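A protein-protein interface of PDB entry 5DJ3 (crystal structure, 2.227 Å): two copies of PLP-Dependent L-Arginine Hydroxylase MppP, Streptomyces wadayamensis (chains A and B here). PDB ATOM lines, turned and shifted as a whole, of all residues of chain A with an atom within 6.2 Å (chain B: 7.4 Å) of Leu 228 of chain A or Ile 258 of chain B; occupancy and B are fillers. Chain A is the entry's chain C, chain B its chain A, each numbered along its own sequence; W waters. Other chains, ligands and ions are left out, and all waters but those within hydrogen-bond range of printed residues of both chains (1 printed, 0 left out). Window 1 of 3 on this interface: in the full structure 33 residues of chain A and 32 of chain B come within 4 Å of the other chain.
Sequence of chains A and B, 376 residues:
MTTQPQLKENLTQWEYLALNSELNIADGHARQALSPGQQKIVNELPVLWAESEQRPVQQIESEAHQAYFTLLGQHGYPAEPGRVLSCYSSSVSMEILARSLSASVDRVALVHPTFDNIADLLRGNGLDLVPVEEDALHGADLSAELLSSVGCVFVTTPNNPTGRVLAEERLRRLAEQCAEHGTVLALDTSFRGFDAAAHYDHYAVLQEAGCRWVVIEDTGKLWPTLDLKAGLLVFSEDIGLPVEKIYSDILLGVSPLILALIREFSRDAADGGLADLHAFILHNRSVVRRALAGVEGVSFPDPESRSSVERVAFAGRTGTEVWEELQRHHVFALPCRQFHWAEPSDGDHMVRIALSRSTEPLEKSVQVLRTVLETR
OH of Tyr 88 of chain B is in hydrogen-bond range of NZ of Lys 229 of chain A, 3.1 Å away.
The side-chain hydroxyl (OG) of Ser 255 of chain B lies within hydrogen-bond range of the backbone carbonyl oxygen (O) of Leu 226 of chain A, 2.8 Å away.
O of Pro 256 of chain B lies close to OG of Ser 52 of chain B, at 3.3 Å.
OG of Ser 52 of chain B sits at hydrogen-bond distance from N of Leu 257 of chain B.
The side-chain hydroxyl (OG) of Ser 255 of chain B lies within hydrogen-bond range of the backbone NH (N) of Leu 257 of chain B (2.9 Å).
OG of Ser 255 of chain B lies within hydrogen-bond range of N of Ile 258 of chain B (3.4 Å).
The side-chain hydroxyl of Thr 225 of chain A is in hydrogen-bond range of the backbone carbonyl oxygen of Leu 228 of chain A (2.7 Å).
The side-chain carboxylate (OD1) of Asp 227 of chain A is in salt-bridge range of the side-chain amino group (NZ) of Lys 229 of chain A.
Among the printed residues, pairs that only touch across the chains: Leu 45 of chain A with Leu 45 of chain B (3.9 Å), Leu 45 of chain A with Trp 49 of chain B (3.8 Å), Thr 225 of chain A with Trp 49 of chain B (3.7 Å), Leu 226 of chain A with Trp 49 of chain B (3.5 Å), Leu 226 of chain A with Ser 52 of chain B (3.6 Å), Leu 226 of chain A with Pro 256 of chain B (3.6 Å), Leu 228 of chain A with Trp 49 of chain B (3.8 Å), Leu 228 of chain A with Ser 255 of chain B (3.6 Å), Leu 228 of chain A with Leu 257 of chain B (3.6 Å), Leu 228 of chain A with Ile 258 of chain B (3.9 Å) and Ile 258 of chain A with Leu 228 of chain B (3.9 Å).
Of chain B, only Trp 49, Ser 255, Leu 257 and Ile 258 come within 4 Å of Leu 228 of chain A.
Of the printed residues of chain B, Lys 229 of chain A touches Tyr 88.
Of the printed residues of chain A, Leu 45 of chain B touches Leu 45.
Of the printed residues of chain A, Pro 256 of chain B touches Leu 226.
Ile 258 of chain B touches just one residue of chain A: Leu 228.
The nearest residue of chain B that does not touch Leu 228 of chain A is Leu 228 of chain B (4.8 Å).
The nearest residue of chain A that does not touch Ile 258 of chain B is Ile 258 of chain A (4.7 Å).
Hydrophobic or aromatic side chains of chain B within 4 Å of the printed part of chain A: Leu 45, Trp 49, Tyr 88, Leu 228, Pro 256, Leu 257 and Ile 258.
Among the printed residues, no Asp or Glu carboxylate lies within 4 Å of a Lys or Arg side-chain nitrogen of the other chain.
Leu 45 of chain B touches its own counterpart, Leu 45 of chain A.
Leu 228 of chain A touches Ile 258 of chain B, and with the chains exchanged Ile 258 of chain A touches Leu 228 of chain B.
Water W1 lies within hydrogen-bond range of NZ of Lys 229 of chain A (2.7 Å), OH of Tyr 88 of chain B (2.8 Å) and OD1 of Asp 227 of chain A (3.2 Å).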
ATOM      1  N   LEU A  45     -29.308 -13.111  -8.342  1.00  0.00           N
ATOM      2  CA  LEU A  45     -28.423 -12.288  -9.154  1.00  0.00           C
ATOM      3  C   LEU A  45     -29.153 -11.185  -9.887  1.00  0.00           C
ATOM      4  O   LEU A  45     -28.566 -10.104 -10.031  1.00  0.00           O
ATOM      5  CB  LEU A  45     -27.656 -13.158 -10.158  1.00  0.00           C
ATOM      6  CG  LEU A  45     -26.335 -13.703  -9.639  1.00  0.00           C
ATOM      7  CD1 LEU A  45     -25.843 -14.848 -10.508  1.00  0.00           C
ATOM      8  CD2 LEU A  45     -25.308 -12.581  -9.572  1.00  0.00           C
ATOM      9  N   THR A 219     -10.570 -12.516  -2.573  1.00  0.00           N
ATOM     10  CA  THR A 219     -11.787 -13.285  -2.319  1.00  0.00           C
ATOM     11  C   THR A 219     -11.849 -14.572  -3.134  1.00  0.00           C
ATOM     12  O   THR A 219     -12.705 -15.420  -2.860  1.00  0.00           O
ATOM     13  CB  THR A 219     -13.058 -12.455  -2.616  1.00  0.00           C
ATOM     14  OG1 THR A 219     -13.225 -12.269  -4.035  1.00  0.00           O
ATOM     15  CG2 THR A 219     -12.997 -11.090  -1.949  1.00  0.00           C
ATOM     16  N   GLY A 220     -10.921 -14.775  -4.065  1.00  0.00           N
ATOM     17  CA  GLY A 220     -11.113 -15.733  -5.149  1.00  0.00           C
ATOM     18  C   GLY A 220     -10.871 -17.200  -4.836  1.00  0.00           C
ATOM     19  O   GLY A 220     -11.234 -18.043  -5.659  1.00  0.00           O
ATOM     20  N   TRP A 223     -14.601 -19.326  -2.286  1.00  0.00           N
ATOM     21  CA  TRP A 223     -15.904 -19.824  -2.687  1.00  0.00           C
ATOM     22  C   TRP A 223     -15.922 -20.208  -4.155  1.00  0.00           C
ATOM     23  O   TRP A 223     -15.096 -19.736  -4.935  1.00  0.00           O
ATOM     24  CB  TRP A 223     -16.980 -18.767  -2.420  1.00  0.00           C
ATOM     25  CG  TRP A 223     -16.983 -18.231  -1.017  1.00  0.00           C
ATOM     26  CD1 TRP A 223     -17.172 -18.938   0.134  1.00  0.00           C
ATOM     27  CD2 TRP A 223     -16.829 -16.860  -0.625  1.00  0.00           C
ATOM     28  NE1 TRP A 223     -17.138 -18.098   1.215  1.00  0.00           N
ATOM     29  CE2 TRP A 223     -16.942 -16.813   0.777  1.00  0.00           C
ATOM     30  CE3 TRP A 223     -16.616 -15.674  -1.322  1.00  0.00           C
ATOM     31  CZ2 TRP A 223     -16.839 -15.621   1.495  1.00  0.00           C
ATOM     32  CZ3 TRP A 223     -16.516 -14.490  -0.604  1.00  0.00           C
ATOM     33  CH2 TRP A 223     -16.619 -14.475   0.786  1.00  0.00           C
ATOM     34  N   THR A 225     -17.261 -19.249  -7.036  1.00  0.00           N
ATOM     35  CA  THR A 225     -17.971 -18.152  -7.670  1.00  0.00           C
ATOM     36  C   THR A 225     -17.553 -17.981  -9.121  1.00  0.00           C
ATOM     37  O   THR A 225     -17.576 -16.866  -9.650  1.00  0.00           O
ATOM     38  CB  THR A 225     -17.731 -16.854  -6.908  1.00  0.00           C
ATOM     39  OG1 THR A 225     -16.337 -16.648  -6.794  1.00  0.00           O
ATOM     40  CG2 THR A 225     -18.317 -16.904  -5.534  1.00  0.00           C
ATOM     41  N   LEU A 226     -17.132 -19.077  -9.757  1.00  0.00           N
ATOM     42  CA  LEU A 226     -16.783 -19.069 -11.169  1.00  0.00           C
ATOM     43  C   LEU A 226     -15.791 -17.950 -11.496  1.00  0.00           C
ATOM     44  O   LEU A 226     -15.921 -17.247 -12.495  1.00  0.00           O
ATOM     45  CB  LEU A 226     -18.035 -18.937 -12.029  1.00  0.00           C
ATOM     46  CG  LEU A 226     -19.052 -20.003 -11.729  1.00  0.00           C
ATOM     47  CD1 LEU A 226     -20.322 -19.644 -12.419  1.00  0.00           C
ATOM     48  CD2 LEU A 226     -18.528 -21.342 -12.187  1.00  0.00           C
ATOM     49  N   ASP A 227     -14.778 -17.795 -10.659  1.00  0.00           N
ATOM     50  CA  ASP A 227     -13.740 -16.787 -10.865  1.00  0.00           C
ATOM     51  C   ASP A 227     -14.283 -15.351 -10.839  1.00  0.00           C
ATOM     52  O   ASP A 227     -13.592 -14.408 -11.281  1.00  0.00           O
ATOM     53  CB  ASP A 227     -12.980 -17.044 -12.158  1.00  0.00           C
ATOM     54  CG  ASP A 227     -11.755 -17.901 -11.925  1.00  0.00           C
ATOM     55  OD1 ASP A 227     -10.867 -17.432 -11.178  1.00  0.00           O
ATOM     56  OD2 ASP A 227     -11.684 -19.028 -12.464  1.00  0.00           O
ATOM     57  N   LEU A 228     -15.500 -15.171 -10.327  1.00  0.00           N
ATOM     58  CA  LEU A 228     -15.962 -13.853  -9.926  1.00  0.00           C
ATOM     59  C   LEU A 228     -15.372 -13.522  -8.569  1.00  0.00           C
ATOM     60  O   LEU A 228     -15.679 -14.174  -7.565  1.00  0.00           O
ATOM     61  CB  LEU A 228     -17.479 -13.800  -9.875  1.00  0.00           C
ATOM     62  CG  LEU A 228     -18.082 -14.126 -11.227  1.00  0.00           C
ATOM     63  CD1 LEU A 228     -19.602 -14.255 -11.031  1.00  0.00           C
ATOM     64  CD2 LEU A 228     -17.680 -13.067 -12.222  1.00  0.00           C
ATOM     65  N   LYS A 229     -14.534 -12.497  -8.533  1.00  0.00           N
ATOM     66  CA  LYS A 229     -13.689 -12.281  -7.371  1.00  0.00           C
ATOM     67  C   LYS A 229     -13.147 -10.865  -7.444  1.00  0.00           C
ATOM     68  O   LYS A 229     -13.379 -10.145  -8.416  1.00  0.00           O
ATOM     69  CB  LYS A 229     -12.559 -13.312  -7.357  1.00  0.00           C
ATOM     70  CG  LYS A 229     -11.707 -13.216  -8.623  1.00  0.00           C
ATOM     71  CD  LYS A 229     -10.649 -14.301  -8.836  1.00  0.00           C
ATOM     72  CE  LYS A 229     -10.066 -14.092 -10.231  1.00  0.00           C
ATOM     73  NZ  LYS A 229      -9.164 -15.159 -10.726  1.00  0.00           N
ATOM     74  N   ALA A 230     -12.364 -10.502  -6.429  1.00  0.00           N
ATOM     75  CA  ALA A 230     -11.560  -9.286  -6.443  1.00  0.00           C
ATOM     76  C   ALA A 230     -10.288  -9.515  -5.638  1.00  0.00           C
ATOM     77  O   ALA A 230     -10.323 -10.141  -4.571  1.00  0.00           O
ATOM     78  CB  ALA A 230     -12.326  -8.096  -5.855  1.00  0.00           C
ATOM     79  N   ILE A 258     -20.023  -7.864  -8.871  1.00  0.00           N
ATOM     80  CA  ILE A 258     -19.066  -8.743  -8.197  1.00  0.00           C
ATOM     81  C   ILE A 258     -18.892  -8.308  -6.748  1.00  0.00           C
ATOM     82  O   ILE A 258     -18.867  -9.143  -5.834  1.00  0.00           O
ATOM     83  CB  ILE A 258     -17.722  -8.779  -8.968  1.00  0.00           C
ATOM     84  CG1 ILE A 258     -17.848  -9.614 -10.239  1.00  0.00           C
ATOM     85  CG2 ILE A 258     -16.601  -9.369  -8.110  1.00  0.00           C
ATOM     86  CD1 ILE A 258     -16.584  -9.544 -11.179  1.00  0.00           C
ATOM     87  N   LEU A 261     -21.955  -9.429  -4.967  1.00  0.00           N
ATOM     88  CA  LEU A 261     -21.742 -10.858  -4.772  1.00  0.00           C
ATOM     89  C   LEU A 261     -20.824 -11.150  -3.586  1.00  0.00           C
ATOM     90  O   LEU A 261     -21.132 -11.993  -2.730  1.00  0.00           O
ATOM     91  CB  LEU A 261     -21.139 -11.436  -6.046  1.00  0.00           C
ATOM     92  CG  LEU A 261     -21.283 -12.917  -6.188  1.00  0.00           C
ATOM     93  CD1 LEU A 261     -22.746 -13.228  -6.415  1.00  0.00           C
ATOM     94  CD2 LEU A 261     -20.455 -13.371  -7.358  1.00  0.00           C
ATOM     95  N   ILE A 262     -19.665 -10.487  -3.550  1.00  0.00           N
ATOM     96  CA  ILE A 262     -18.726 -10.659  -2.445  1.00  0.00           C
ATOM     97  C   ILE A 262     -19.406 -10.305  -1.125  1.00  0.00           C
ATOM     98  O   ILE A 262     -19.322 -11.047  -0.139  1.00  0.00           O
ATOM     99  CB  ILE A 262     -17.462  -9.804  -2.692  1.00  0.00           C
ATOM    100  CG1 ILE A 262     -16.639 -10.401  -3.829  1.00  0.00           C
ATOM    101  CG2 ILE A 262     -16.611  -9.617  -1.422  1.00  0.00           C
ATOM    102  CD1 ILE A 262     -15.582  -9.441  -4.410  1.00  0.00           C
ATOM    103  N   LEU B  45     -29.527 -15.027 -15.360  1.00  0.00           N
ATOM    104  CA  LEU B  45     -28.195 -15.193 -14.785  1.00  0.00           C
ATOM    105  C   LEU B  45     -28.056 -16.466 -13.963  1.00  0.00           C
ATOM    106  O   LEU B  45     -27.008 -17.119 -14.068  1.00  0.00           O
ATOM    107  CB  LEU B  45     -27.840 -13.968 -13.945  1.00  0.00           C
ATOM    108  CG  LEU B  45     -27.100 -12.895 -14.709  1.00  0.00           C
ATOM    109  CD1 LEU B  45     -26.967 -11.706 -13.772  1.00  0.00           C
ATOM    110  CD2 LEU B  45     -25.734 -13.370 -15.175  1.00  0.00           C
ATOM    111  N   TRP B  49     -25.221 -19.275 -14.799  1.00  0.00           N
ATOM    112  CA  TRP B  49     -24.372 -19.796 -13.730  1.00  0.00           C
ATOM    113  C   TRP B  49     -24.316 -21.316 -13.757  1.00  0.00           C
ATOM    114  O   TRP B  49     -23.231 -21.915 -13.716  1.00  0.00           O
ATOM    115  CB  TRP B  49     -24.891 -19.354 -12.362  1.00  0.00           C
ATOM    116  CG  TRP B  49     -23.952 -19.665 -11.279  1.00  0.00           C
ATOM    117  CD1 TRP B  49     -23.666 -20.894 -10.797  1.00  0.00           C
ATOM    118  CD2 TRP B  49     -23.171 -18.738 -10.521  1.00  0.00           C
ATOM    119  NE1 TRP B  49     -22.736 -20.804  -9.806  1.00  0.00           N
ATOM    120  CE2 TRP B  49     -22.424 -19.486  -9.606  1.00  0.00           C
ATOM    121  CE3 TRP B  49     -23.021 -17.344 -10.535  1.00  0.00           C
ATOM    122  CZ2 TRP B  49     -21.555 -18.896  -8.702  1.00  0.00           C
ATOM    123  CZ3 TRP B  49     -22.141 -16.766  -9.646  1.00  0.00           C
ATOM    124  CH2 TRP B  49     -21.426 -17.540  -8.741  1.00  0.00           C
ATOM    125  N   SER B  52     -22.322 -22.442 -16.595  1.00  0.00           N
ATOM    126  CA  SER B  52     -20.894 -22.232 -16.363  1.00  0.00           C
ATOM    127  C   SER B  52     -20.306 -23.291 -15.448  1.00  0.00           C
ATOM    128  O   SER B  52     -19.150 -23.682 -15.618  1.00  0.00           O
ATOM    129  CB  SER B  52     -20.663 -20.857 -15.758  1.00  0.00           C
ATOM    130  OG  SER B  52     -20.940 -19.872 -16.696  1.00  0.00           O
ATOM    131  N   ILE B  60     -17.365 -22.574 -23.587  1.00  0.00           N
ATOM    132  CA  ILE B  60     -18.124 -21.341 -23.466  1.00  0.00           C
ATOM    133  C   ILE B  60     -17.312 -20.205 -24.042  1.00  0.00           C
ATOM    134  O   ILE B  60     -17.848 -19.332 -24.734  1.00  0.00           O
ATOM    135  CB  ILE B  60     -18.529 -21.061 -21.999  1.00  0.00           C
ATOM    136  CG1 ILE B  60     -19.500 -22.113 -21.473  1.00  0.00           C
ATOM    137  CG2 ILE B  60     -19.235 -19.722 -21.893  1.00  0.00           C
ATOM    138  CD1 ILE B  60     -19.764 -22.019 -19.982  1.00  0.00           C
ATOM    139  N   ALA B  64     -18.359 -17.581 -26.851  1.00  0.00           N
ATOM    140  CA  ALA B  64     -18.334 -16.146 -26.602  1.00  0.00           C
ATOM    141  C   ALA B  64     -17.532 -15.430 -27.671  1.00  0.00           C
ATOM    142  O   ALA B  64     -17.984 -14.430 -28.249  1.00  0.00           O
ATOM    143  CB  ALA B  64     -17.747 -15.869 -25.229  1.00  0.00           C
ATOM    144  N   CYS B  87      -8.963 -11.772 -21.222  1.00  0.00           N
ATOM    145  CA  CYS B  87      -8.413 -11.065 -20.078  1.00  0.00           C
ATOM    146  C   CYS B  87      -9.529 -10.311 -19.351  1.00  0.00           C
ATOM    147  O   CYS B  87     -10.578 -10.039 -19.920  1.00  0.00           O
ATOM    148  CB  CYS B  87      -7.313 -10.056 -20.513  1.00  0.00           C
ATOM    149  SG  CYS B  87      -6.066 -10.657 -21.742  1.00  0.00           S
ATOM    150  N   TYR B  88      -9.289  -9.943 -18.087  1.00  0.00           N
ATOM    151  CA  TYR B  88     -10.317  -9.256 -17.310  1.00  0.00           C
ATOM    152  C   TYR B  88     -10.748  -7.955 -17.958  1.00  0.00           C
ATOM    153  O   TYR B  88     -11.867  -7.494 -17.717  1.00  0.00           O
ATOM    154  CB  TYR B  88      -9.827  -8.965 -15.892  1.00  0.00           C
ATOM    155  CG  TYR B  88      -9.316 -10.180 -15.141  1.00  0.00           C
ATOM    156  CD1 TYR B  88     -10.158 -11.225 -14.848  1.00  0.00           C
ATOM    157  CD2 TYR B  88      -7.999 -10.269 -14.724  1.00  0.00           C
ATOM    158  CE1 TYR B  88      -9.734 -12.325 -14.145  1.00  0.00           C
ATOM    159  CE2 TYR B  88      -7.555 -11.386 -14.034  1.00  0.00           C
ATOM    160  CZ  TYR B  88      -8.433 -12.403 -13.738  1.00  0.00           C
ATOM    161  OH  TYR B  88      -8.012 -13.515 -13.023  1.00  0.00           O
ATOM    162  N   THR B 219     -15.066  -6.033 -24.882  1.00  0.00           N
ATOM    163  CA  THR B 219     -16.517  -6.059 -24.798  1.00  0.00           C
ATOM    164  C   THR B 219     -17.085  -5.010 -23.849  1.00  0.00           C
ATOM    165  O   THR B 219     -18.301  -4.794 -23.846  1.00  0.00           O
ATOM    166  CB  THR B 219     -17.021  -7.432 -24.335  1.00  0.00           C
ATOM    167  OG1 THR B 219     -16.737  -7.613 -22.942  1.00  0.00           O
ATOM    168  CG2 THR B 219     -16.376  -8.578 -25.143  1.00  0.00           C
ATOM    169  N   ASP B 227     -19.595  -3.419 -15.961  1.00  0.00           N
ATOM    170  CA  ASP B 227     -18.177  -3.744 -16.057  1.00  0.00           C
ATOM    171  C   ASP B 227     -17.894  -5.235 -16.036  1.00  0.00           C
ATOM    172  O   ASP B 227     -16.759  -5.650 -15.771  1.00  0.00           O
ATOM    173  CB  ASP B 227     -17.372  -3.056 -14.956  1.00  0.00           C
ATOM    174  CG  ASP B 227     -16.787  -1.774 -15.428  1.00  0.00           C
ATOM    175  OD1 ASP B 227     -16.070  -1.832 -16.452  1.00  0.00           O
ATOM    176  OD2 ASP B 227     -17.074  -0.722 -14.817  1.00  0.00           O
ATOM    177  N   LEU B 228     -18.899  -6.052 -16.291  1.00  0.00           N
ATOM    178  CA  LEU B 228     -18.654  -7.451 -16.619  1.00  0.00           C
ATOM    179  C   LEU B 228     -18.288  -7.498 -18.096  1.00  0.00           C
ATOM    180  O   LEU B 228     -19.118  -7.200 -18.966  1.00  0.00           O
ATOM    181  CB  LEU B 228     -19.868  -8.313 -16.305  1.00  0.00           C
ATOM    182  CG  LEU B 228     -20.326  -8.187 -14.847  1.00  0.00           C
ATOM    183  CD1 LEU B 228     -21.720  -8.709 -14.695  1.00  0.00           C
ATOM    184  CD2 LEU B 228     -19.345  -8.921 -13.913  1.00  0.00           C
ATOM    185  N   LYS B 229     -17.055  -7.888 -18.378  1.00  0.00           N
ATOM    186  CA  LYS B 229     -16.464  -7.664 -19.682  1.00  0.00           C
ATOM    187  C   LYS B 229     -15.225  -8.540 -19.823  1.00  0.00           C
ATOM    188  O   LYS B 229     -14.758  -9.146 -18.861  1.00  0.00           O
ATOM    189  CB  LYS B 229     -16.110  -6.193 -19.807  1.00  0.00           C
ATOM    190  CG  LYS B 229     -15.105  -5.826 -18.754  1.00  0.00           C
ATOM    191  CD  LYS B 229     -14.867  -4.388 -18.658  1.00  0.00           C
ATOM    192  CE  LYS B 229     -14.020  -4.083 -17.445  1.00  0.00           C
ATOM    193  NZ  LYS B 229     -13.784  -2.633 -17.335  1.00  0.00           N
ATOM    194  N   ALA B 230     -14.695  -8.598 -21.035  1.00  0.00           N
ATOM    195  CA  ALA B 230     -13.403  -9.220 -21.291  1.00  0.00           C
ATOM    196  C   ALA B 230     -12.609  -8.360 -22.264  1.00  0.00           C
ATOM    197  O   ALA B 230     -13.160  -7.820 -23.225  1.00  0.00           O
ATOM    198  CB  ALA B 230     -13.545 -10.628 -21.881  1.00  0.00           C
ATOM    199  N   VAL B 254     -10.862 -15.913 -17.756  1.00  0.00           N
ATOM    200  CA  VAL B 254     -11.907 -15.083 -17.182  1.00  0.00           C
ATOM    201  C   VAL B 254     -13.094 -15.959 -16.817  1.00  0.00           C
ATOM    202  O   VAL B 254     -13.244 -17.083 -17.305  1.00  0.00           O
ATOM    203  CB  VAL B 254     -12.331 -13.964 -18.140  1.00  0.00           C
ATOM    204  CG1 VAL B 254     -11.113 -13.123 -18.500  1.00  0.00           C
ATOM    205  CG2 VAL B 254     -12.996 -14.547 -19.378  1.00  0.00           C
ATOM    206  N   SER B 255     -13.968 -15.409 -15.971  1.00  0.00           N
ATOM    207  CA  SER B 255     -15.093 -16.159 -15.447  1.00  0.00           C
ATOM    208  C   SER B 255     -15.919 -16.740 -16.588  1.00  0.00           C
ATOM    209  O   SER B 255     -16.200 -16.036 -17.559  1.00  0.00           O
ATOM    210  CB  SER B 255     -15.979 -15.268 -14.573  1.00  0.00           C
ATOM    211  OG  SER B 255     -17.307 -15.813 -14.475  1.00  0.00           O
ATOM    212  N   PRO B 256     -16.316 -18.010 -16.519  1.00  0.00           N
ATOM    213  CA  PRO B 256     -17.264 -18.516 -17.523  1.00  0.00           C
ATOM    214  C   PRO B 256     -18.602 -17.775 -17.512  1.00  0.00           C
ATOM    215  O   PRO B 256     -19.263 -17.696 -18.562  1.00  0.00           O
ATOM    216  CB  PRO B 256     -17.442 -19.994 -17.148  1.00  0.00           C
ATOM    217  CG  PRO B 256     -16.471 -20.290 -16.099  1.00  0.00           C
ATOM    218  CD  PRO B 256     -15.843 -19.047 -15.592  1.00  0.00           C
ATOM    219  N   LEU B 257     -19.038 -17.266 -16.356  1.00  0.00           N
ATOM    220  CA  LEU B 257     -20.273 -16.501 -16.325  1.00  0.00           C
ATOM    221  C   LEU B 257     -20.161 -15.238 -17.178  1.00  0.00           C
ATOM    222  O   LEU B 257     -21.103 -14.886 -17.898  1.00  0.00           O
ATOM    223  CB  LEU B 257     -20.654 -16.156 -14.886  1.00  0.00           C
ATOM    224  CG  LEU B 257     -22.036 -15.507 -14.752  1.00  0.00           C
ATOM    225  CD1 LEU B 257     -23.091 -16.525 -15.022  1.00  0.00           C
ATOM    226  CD2 LEU B 257     -22.282 -14.887 -13.381  1.00  0.00           C
ATOM    227  N   ILE B 258     -18.994 -14.571 -17.156  1.00  0.00           N
ATOM    228  CA  ILE B 258     -18.834 -13.364 -17.958  1.00  0.00           C
ATOM    229  C   ILE B 258     -18.781 -13.708 -19.454  1.00  0.00           C
ATOM    230  O   ILE B 258     -19.411 -13.033 -20.280  1.00  0.00           O
ATOM    231  CB  ILE B 258     -17.585 -12.581 -17.511  1.00  0.00           C
ATOM    232  CG1 ILE B 258     -17.811 -11.989 -16.129  1.00  0.00           C
ATOM    233  CG2 ILE B 258     -17.254 -11.476 -18.520  1.00  0.00           C
ATOM    234  CD1 ILE B 258     -16.595 -11.380 -15.518  1.00  0.00           C
ATOM    235  N   LEU B 259     -18.031 -14.755 -19.823  1.00  0.00           N
ATOM    236  CA  LEU B 259     -18.022 -15.226 -21.212  1.00  0.00           C
ATOM    237  C   LEU B 259     -19.432 -15.609 -21.667  1.00  0.00           C
ATOM    238  O   LEU B 259     -19.836 -15.262 -22.789  1.00  0.00           O
ATOM    239  CB  LEU B 259     -17.070 -16.399 -21.369  1.00  0.00           C
ATOM    240  CG  LEU B 259     -15.591 -16.045 -21.111  1.00  0.00           C
ATOM    241  CD1 LEU B 259     -14.714 -17.268 -20.929  1.00  0.00           C
ATOM    242  CD2 LEU B 259     -15.038 -15.181 -22.221  1.00  0.00           C
ATOM    243  N   ALA B 260     -20.218 -16.266 -20.791  1.00  0.00           N
ATOM    244  CA  ALA B 260     -21.581 -16.623 -21.163  1.00  0.00           C
ATOM    245  C   ALA B 260     -22.409 -15.370 -21.403  1.00  0.00           C
ATOM    246  O   ALA B 260     -23.150 -15.291 -22.381  1.00  0.00           O
ATOM    247  CB  ALA B 260     -22.231 -17.497 -20.084  1.00  0.00           C
ATOM    248  N   LEU B 261     -22.241 -14.365 -20.542  1.00  0.00           N
ATOM    249  CA  LEU B 261     -22.938 -13.101 -20.694  1.00  0.00           C
ATOM    250  C   LEU B 261     -22.537 -12.409 -21.998  1.00  0.00           C
ATOM    251  O   LEU B 261     -23.396 -11.957 -22.775  1.00  0.00           O
ATOM    252  CB  LEU B 261     -22.644 -12.226 -19.483  1.00  0.00           C
ATOM    253  CG  LEU B 261     -23.604 -11.075 -19.194  1.00  0.00           C
ATOM    254  CD1 LEU B 261     -24.985 -11.610 -18.751  1.00  0.00           C
ATOM    255  CD2 LEU B 261     -23.037 -10.147 -18.129  1.00  0.00           C
ATOM    256  N   ILE B 262     -21.237 -12.361 -22.287  1.00  0.00           N
ATOM    257  CA  ILE B 262     -20.801 -11.795 -23.562  1.00  0.00           C
ATOM    258  C   ILE B 262     -21.491 -12.510 -24.709  1.00  0.00           C
ATOM    259  O   ILE B 262     -21.981 -11.886 -25.652  1.00  0.00           O
ATOM    260  CB  ILE B 262     -19.275 -11.897 -23.712  1.00  0.00           C
ATOM    261  CG1 ILE B 262     -18.566 -10.910 -22.785  1.00  0.00           C
ATOM    262  CG2 ILE B 262     -18.865 -11.642 -25.168  1.00  0.00           C
ATOM    263  CD1 ILE B 262     -17.130 -11.381 -22.450  1.00  0.00           C
ATOM    264  N   ARG B 263     -21.499 -13.841 -24.655  1.00  0.00           N
ATOM    265  CA  ARG B 263     -22.113 -14.644 -25.706  1.00  0.00           C
ATOM    266  C   ARG B 263     -23.576 -14.263 -25.908  1.00  0.00           C
ATOM    267  O   ARG B 263     -24.033 -14.106 -27.049  1.00  0.00           O
ATOM    268  CB  ARG B 263     -21.998 -16.131 -25.355  1.00  0.00           C
ATOM    269  CG  ARG B 263     -22.526 -17.069 -26.448  1.00  0.00           C
ATOM    270  CD  ARG B 263     -22.782 -18.457 -25.867  1.00  0.00           C
ATOM    271  NE  ARG B 263     -23.765 -18.444 -24.783  1.00  0.00           N
ATOM    272  CZ  ARG B 263     -23.848 -19.388 -23.847  1.00  0.00           C
ATOM    273  NH1 ARG B 263     -23.005 -20.422 -23.849  1.00  0.00           N
ATOM    274  NH2 ARG B 263     -24.775 -19.292 -22.899  1.00  0.00           N
ATOM    275  N   GLU B 264     -24.321 -14.115 -24.803  1.00  0.00           N
ATOM    276  CA  GLU B 264     -25.757 -13.825 -24.860  1.00  0.00           C
ATOM    277  C   GLU B 264     -26.004 -12.383 -25.282  1.00  0.00           C
ATOM    278  O   GLU B 264     -26.919 -12.106 -26.071  1.00  0.00           O
ATOM    279  CB  GLU B 264     -26.416 -14.097 -23.500  1.00  0.00           C
ATOM    280  CG  GLU B 264     -26.462 -15.559 -23.085  1.00  0.00           C
ATOM    281  CD  GLU B 264     -27.032 -16.452 -24.187  1.00  0.00           C
ATOM    282  OE1 GLU B 264     -28.086 -16.073 -24.752  1.00  0.00           O
ATOM    283  OE2 GLU B 264     -26.407 -17.507 -24.508  1.00  0.00           O
ATOM    284  N   PHE B 265     -25.201 -11.449 -24.771  1.00  0.00           N
ATOM    285  CA  PHE B 265     -25.359 -10.059 -25.199  1.00  0.00           C
ATOM    286  C   PHE B 265     -24.999  -9.883 -26.676  1.00  0.00           C
ATOM    287  O   PHE B 265     -25.626  -9.076 -27.371  1.00  0.00           O
ATOM    288  CB  PHE B 265     -24.512  -9.134 -24.322  1.00  0.00           C
ATOM    289  CG  PHE B 265     -25.248  -8.582 -23.158  1.00  0.00           C
ATOM    290  CD1 PHE B 265     -25.511  -9.369 -22.050  1.00  0.00           C
ATOM    291  CD2 PHE B 265     -25.694  -7.273 -23.163  1.00  0.00           C
ATOM    292  CE1 PHE B 265     -26.225  -8.849 -20.976  1.00  0.00           C
ATOM    293  CE2 PHE B 265     -26.400  -6.759 -22.090  1.00  0.00           C
ATOM    294  CZ  PHE B 265     -26.661  -7.553 -21.000  1.00  0.00           C
HETATM  295  O   HOH W   1      -8.770 -16.198 -13.227  1.00  0.00           O
